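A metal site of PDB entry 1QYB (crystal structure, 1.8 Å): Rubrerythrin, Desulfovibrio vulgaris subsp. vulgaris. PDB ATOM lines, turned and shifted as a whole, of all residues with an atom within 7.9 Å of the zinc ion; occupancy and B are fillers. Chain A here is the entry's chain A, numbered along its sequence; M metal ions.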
ATOM      1  N   ARG A 157     -16.052  -4.387   4.486  1.00  0.00           N
ATOM      2  CA  ARG A 157     -16.153  -4.670   3.057  1.00  0.00           C
ATOM      3  C   ARG A 157     -15.302  -3.698   2.237  1.00  0.00           C
ATOM      4  O   ARG A 157     -15.283  -2.502   2.510  1.00  0.00           O
ATOM      5  CB  ARG A 157     -17.605  -4.585   2.579  1.00  0.00           C
ATOM      6  CG  ARG A 157     -17.814  -5.063   1.143  1.00  0.00           C
ATOM      7  CD  ARG A 157     -19.235  -4.828   0.640  1.00  0.00           C
ATOM      8  NE  ARG A 157     -19.506  -3.408   0.398  1.00  0.00           N
ATOM      9  CZ  ARG A 157     -19.885  -2.915  -0.779  1.00  0.00           C
ATOM     10  NH1 ARG A 157     -20.024  -3.712  -1.824  1.00  0.00           N
ATOM     11  NH2 ARG A 157     -20.118  -1.615  -0.903  1.00  0.00           N
ATOM     12  N   CYS A 158     -14.585  -4.239   1.258  1.00  0.00           N
ATOM     13  CA  CYS A 158     -13.770  -3.402   0.387  1.00  0.00           C
ATOM     14  C   CYS A 158     -14.703  -2.824  -0.675  1.00  0.00           C
ATOM     15  O   CYS A 158     -15.318  -3.577  -1.428  1.00  0.00           O
ATOM     16  CB  CYS A 158     -12.685  -4.236  -0.310  1.00  0.00           C
ATOM     17  SG  CYS A 158     -11.717  -3.319  -1.554  1.00  0.00           S
ATOM     18  N   ARG A 159     -14.836  -1.497  -0.732  1.00  0.00           N
ATOM     19  CA  ARG A 159     -15.717  -0.888  -1.717  1.00  0.00           C
ATOM     20  C   ARG A 159     -15.200  -1.089  -3.153  1.00  0.00           C
ATOM     21  O   ARG A 159     -15.970  -1.088  -4.105  1.00  0.00           O
ATOM     22  CB  ARG A 159     -15.900   0.608  -1.429  1.00  0.00           C
ATOM     23  CG  ARG A 159     -16.743   0.911  -0.198  1.00  0.00           C
ATOM     24  CD  ARG A 159     -16.951   2.416  -0.016  1.00  0.00           C
ATOM     25  NE  ARG A 159     -17.705   2.996  -1.123  1.00  0.00           N
ATOM     26  CZ  ARG A 159     -19.006   2.788  -1.343  1.00  0.00           C
ATOM     27  NH1 ARG A 159     -19.706   2.023  -0.518  1.00  0.00           N
ATOM     28  NH2 ARG A 159     -19.598   3.347  -2.385  1.00  0.00           N
ATOM     29  N   ASN A 160     -13.893  -1.288  -3.298  1.00  0.00           N
ATOM     30  CA  ASN A 160     -13.328  -1.463  -4.616  1.00  0.00           C
ATOM     31  C   ASN A 160     -13.642  -2.816  -5.271  1.00  0.00           C
ATOM     32  O   ASN A 160     -13.994  -2.854  -6.451  1.00  0.00           O
ATOM     33  CB  ASN A 160     -11.807  -1.249  -4.574  1.00  0.00           C
ATOM     34  CG  ASN A 160     -11.179  -1.239  -5.959  1.00  0.00           C
ATOM     35  OD1 ASN A 160     -10.436  -2.146  -6.330  1.00  0.00           O
ATOM     36  ND2 ASN A 160     -11.490  -0.197  -6.740  1.00  0.00           N
ATOM     37  N   CYS A 161     -13.536  -3.899  -4.506  1.00  0.00           N
ATOM     38  CA  CYS A 161     -13.767  -5.238  -5.072  1.00  0.00           C
ATOM     39  C   CYS A 161     -14.780  -6.111  -4.348  1.00  0.00           C
ATOM     40  O   CYS A 161     -15.113  -7.200  -4.833  1.00  0.00           O
ATOM     41  CB  CYS A 161     -12.450  -5.991  -5.168  1.00  0.00           C
ATOM     42  SG  CYS A 161     -11.875  -6.662  -3.587  1.00  0.00           S
ATOM     43  N   GLY A 162     -15.250  -5.678  -3.181  1.00  0.00           N
ATOM     44  CA  GLY A 162     -16.236  -6.457  -2.452  1.00  0.00           C
ATOM     45  C   GLY A 162     -15.689  -7.465  -1.456  1.00  0.00           C
ATOM     46  O   GLY A 162     -16.455  -8.208  -0.835  1.00  0.00           O
ATOM     47  N   TYR A 163     -14.371  -7.521  -1.316  1.00  0.00           N
ATOM     48  CA  TYR A 163     -13.762  -8.458  -0.371  1.00  0.00           C
ATOM     49  C   TYR A 163     -14.298  -8.146   1.018  1.00  0.00           C
ATOM     50  O   TYR A 163     -14.498  -6.986   1.366  1.00  0.00           O
ATOM     51  CB  TYR A 163     -12.245  -8.317  -0.375  1.00  0.00           C
ATOM     52  CG  TYR A 163     -11.568  -9.226   0.638  1.00  0.00           C
ATOM     53  CD1 TYR A 163     -11.455 -10.594   0.396  1.00  0.00           C
ATOM     54  CD2 TYR A 163     -11.104  -8.716   1.850  1.00  0.00           C
ATOM     55  CE1 TYR A 163     -10.893 -11.437   1.346  1.00  0.00           C
ATOM     56  CE2 TYR A 163     -10.555  -9.564   2.805  1.00  0.00           C
ATOM     57  CZ  TYR A 163     -10.448 -10.916   2.546  1.00  0.00           C
ATOM     58  OH  TYR A 163      -9.901 -11.755   3.504  1.00  0.00           O
ATOM     59  N   VAL A 164     -14.537  -9.188   1.818  1.00  0.00           N
ATOM     60  CA  VAL A 164     -15.031  -9.005   3.173  1.00  0.00           C
ATOM     61  C   VAL A 164     -13.979  -9.482   4.170  1.00  0.00           C
ATOM     62  O   VAL A 164     -13.555 -10.636   4.135  1.00  0.00           O
ATOM     63  CB  VAL A 164     -16.326  -9.799   3.420  1.00  0.00           C
ATOM     64  CG1 VAL A 164     -16.748  -9.683   4.894  1.00  0.00           C
ATOM     65  CG2 VAL A 164     -17.447  -9.271   2.528  1.00  0.00           C
ATOM     66  N   LEU A 173      -4.079  -3.288   3.414  1.00  0.00           N
ATOM     67  CA  LEU A 173      -4.278  -3.501   1.986  1.00  0.00           C
ATOM     68  C   LEU A 173      -5.285  -4.620   1.777  1.00  0.00           C
ATOM     69  O   LEU A 173      -5.298  -5.600   2.529  1.00  0.00           O
ATOM     70  CB  LEU A 173      -2.956  -3.903   1.320  1.00  0.00           C
ATOM     71  CG  LEU A 173      -1.813  -2.884   1.241  1.00  0.00           C
ATOM     72  CD1 LEU A 173      -0.572  -3.563   0.697  1.00  0.00           C
ATOM     73  CD2 LEU A 173      -2.232  -1.715   0.358  1.00  0.00           C
ATOM     74  N   CYS A 174      -6.144  -4.471   0.773  1.00  0.00           N
ATOM     75  CA  CYS A 174      -7.139  -5.509   0.502  1.00  0.00           C
ATOM     76  C   CYS A 174      -6.406  -6.736  -0.028  1.00  0.00           C
ATOM     77  O   CYS A 174      -5.593  -6.632  -0.946  1.00  0.00           O
ATOM     78  CB  CYS A 174      -8.148  -5.033  -0.550  1.00  0.00           C
ATOM     79  SG  CYS A 174      -9.378  -6.307  -0.934  1.00  0.00           S
ATOM     80  N   PRO A 175      -6.666  -7.909   0.570  1.00  0.00           N
ATOM     81  CA  PRO A 175      -5.981  -9.117   0.101  1.00  0.00           C
ATOM     82  C   PRO A 175      -6.406  -9.586  -1.285  1.00  0.00           C
ATOM     83  O   PRO A 175      -5.719 -10.382  -1.920  1.00  0.00           O
ATOM     84  CB  PRO A 175      -6.285 -10.132   1.202  1.00  0.00           C
ATOM     85  CG  PRO A 175      -7.606  -9.696   1.713  1.00  0.00           C
ATOM     86  CD  PRO A 175      -7.473  -8.188   1.764  1.00  0.00           C
ATOM     87  N   ALA A 176      -7.552  -9.096  -1.757  1.00  0.00           N
ATOM     88  CA  ALA A 176      -8.038  -9.462  -3.082  1.00  0.00           C
ATOM     89  C   ALA A 176      -7.581  -8.496  -4.168  1.00  0.00           C
ATOM     90  O   ALA A 176      -6.942  -8.909  -5.136  1.00  0.00           O
ATOM     91  CB  ALA A 176      -9.571  -9.565  -3.077  1.00  0.00           C
ATOM     92  N   CYS A 177      -7.878  -7.207  -4.009  1.00  0.00           N
ATOM     93  CA  CYS A 177      -7.515  -6.227  -5.027  1.00  0.00           C
ATOM     94  C   CYS A 177      -6.294  -5.362  -4.740  1.00  0.00           C
ATOM     95  O   CYS A 177      -5.909  -4.523  -5.563  1.00  0.00           O
ATOM     96  CB  CYS A 177      -8.713  -5.303  -5.307  1.00  0.00           C
ATOM     97  SG  CYS A 177      -9.034  -4.114  -3.978  1.00  0.00           S
ATOM     98  N   ALA A 178      -5.674  -5.549  -3.577  1.00  0.00           N
ATOM     99  CA  ALA A 178      -4.481  -4.813  -3.197  1.00  0.00           C
ATOM    100  C   ALA A 178      -4.644  -3.317  -3.016  1.00  0.00           C
ATOM    101  O   ALA A 178      -3.663  -2.582  -2.956  1.00  0.00           O
ATOM    102  CB  ALA A 178      -3.350  -5.093  -4.201  1.00  0.00           C
ATOM    103  N   HIS A 179      -5.883  -2.832  -2.937  1.00  0.00           N
ATOM    104  CA  HIS A 179      -6.096  -1.412  -2.738  1.00  0.00           C
ATOM    105  C   HIS A 179      -5.943  -1.100  -1.257  1.00  0.00           C
ATOM    106  O   HIS A 179      -6.118  -1.976  -0.407  1.00  0.00           O
ATOM    107  CB  HIS A 179      -7.466  -0.982  -3.251  1.00  0.00           C
ATOM    108  CG  HIS A 179      -7.510  -0.790  -4.732  1.00  0.00           C
ATOM    109  ND1 HIS A 179      -7.080  -1.756  -5.617  1.00  0.00           N
ATOM    110  CD2 HIS A 179      -7.916   0.261  -5.492  1.00  0.00           C
ATOM    111  CE1 HIS A 179      -7.212  -1.314  -6.852  1.00  0.00           C
ATOM    112  NE2 HIS A 179      -7.718  -0.090  -6.800  1.00  0.00           N
ATOM    113  N   PRO A 180      -5.594   0.154  -0.910  1.00  0.00           N
ATOM    114  CA  PRO A 180      -5.422   0.533   0.493  1.00  0.00           C
ATOM    115  C   PRO A 180      -6.647   0.520   1.379  1.00  0.00           C
ATOM    116  O   PRO A 180      -7.793   0.517   0.901  1.00  0.00           O
ATOM    117  CB  PRO A 180      -4.781   1.920   0.399  1.00  0.00           C
ATOM    118  CG  PRO A 180      -5.362   2.463  -0.864  1.00  0.00           C
ATOM    119  CD  PRO A 180      -5.287   1.284  -1.809  1.00  0.00           C
ATOM    120  N   HIS A 183     -10.310   2.156   1.156  1.00  0.00           N
ATOM    121  CA  HIS A 183     -11.492   1.648   0.460  1.00  0.00           C
ATOM    122  C   HIS A 183     -12.470   0.846   1.318  1.00  0.00           C
ATOM    123  O   HIS A 183     -13.557   0.530   0.866  1.00  0.00           O
ATOM    124  CB  HIS A 183     -11.056   0.796  -0.736  1.00  0.00           C
ATOM    125  CG  HIS A 183     -10.356   1.579  -1.794  1.00  0.00           C
ATOM    126  ND1 HIS A 183     -11.007   2.070  -2.908  1.00  0.00           N
ATOM    127  CD2 HIS A 183      -9.074   2.006  -1.891  1.00  0.00           C
ATOM    128  CE1 HIS A 183     -10.155   2.761  -3.651  1.00  0.00           C
ATOM    129  NE2 HIS A 183      -8.977   2.740  -3.048  1.00  0.00           N
ATOM    130  N   PHE A 184     -12.095   0.530   2.551  1.00  0.00           N
ATOM    131  CA  PHE A 184     -12.970  -0.256   3.415  1.00  0.00           C
ATOM    132  C   PHE A 184     -14.041   0.497   4.194  1.00  0.00           C
ATOM    133  O   PHE A 184     -13.855   1.632   4.619  1.00  0.00           O
ATOM    134  CB  PHE A 184     -12.136  -1.093   4.385  1.00  0.00           C
ATOM    135  CG  PHE A 184     -11.469  -2.283   3.759  1.00  0.00           C
ATOM    136  CD1 PHE A 184     -10.258  -2.155   3.092  1.00  0.00           C
ATOM    137  CD2 PHE A 184     -12.080  -3.536   3.809  1.00  0.00           C
ATOM    138  CE1 PHE A 184      -9.657  -3.251   2.488  1.00  0.00           C
ATOM    139  CE2 PHE A 184     -11.497  -4.647   3.204  1.00  0.00           C
ATOM    140  CZ  PHE A 184     -10.280  -4.509   2.544  1.00  0.00           C
HETATM  141 ZN    ZN M   1     -10.565  -5.072  -2.521  1.00  0.00          ZN
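Of the 18 residues printed, 4 come within 4 Å of the zinc ion.
The nearest printed residue that does not touch the zinc ion is Tyr 163 (4.2 Å).
SG of Cys 158 binds the zinc ion (2.3 Å).
The zinc ion is bound by SG of Cys 161, at 2.3 Å.
The side-chain sulfur (SG) of Cys 177 is bound to the zinc ion, 2.3 Å away.
The side-chain sulfur (SG) of Cys 174 binds the zinc ion, 2.3 Å away.
The zinc ion has four donor atoms within binding distance.
The side-chain sulfur (SG) of Cys 158 sits close to the backbone NH (N) of Asn 160.
SG of Cys 177 lies close to OD1 of Asn 160, 3.4 Å away.
The backbone NH (N) of Cys 174 lies within hydrogen-bond range of the backbone carbonyl oxygen (O) of His 179, at 2.8 Å.
O of Tyr 163 lies within hydrogen-bond range of N of Cys 158, at 2.8 Å.
The backbone carbonyl oxygen (O) of Cys 177 is in hydrogen-bond range of a ring nitrogen (ND1) of His 179 (3.0 Å).
The side-chain sulfur of Cys 161 sits close to the backbone NH of Tyr 163, 3.5 Å away.
The side-chain sulfur of Cys 174 lies close to the backbone NH of Ala 176.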
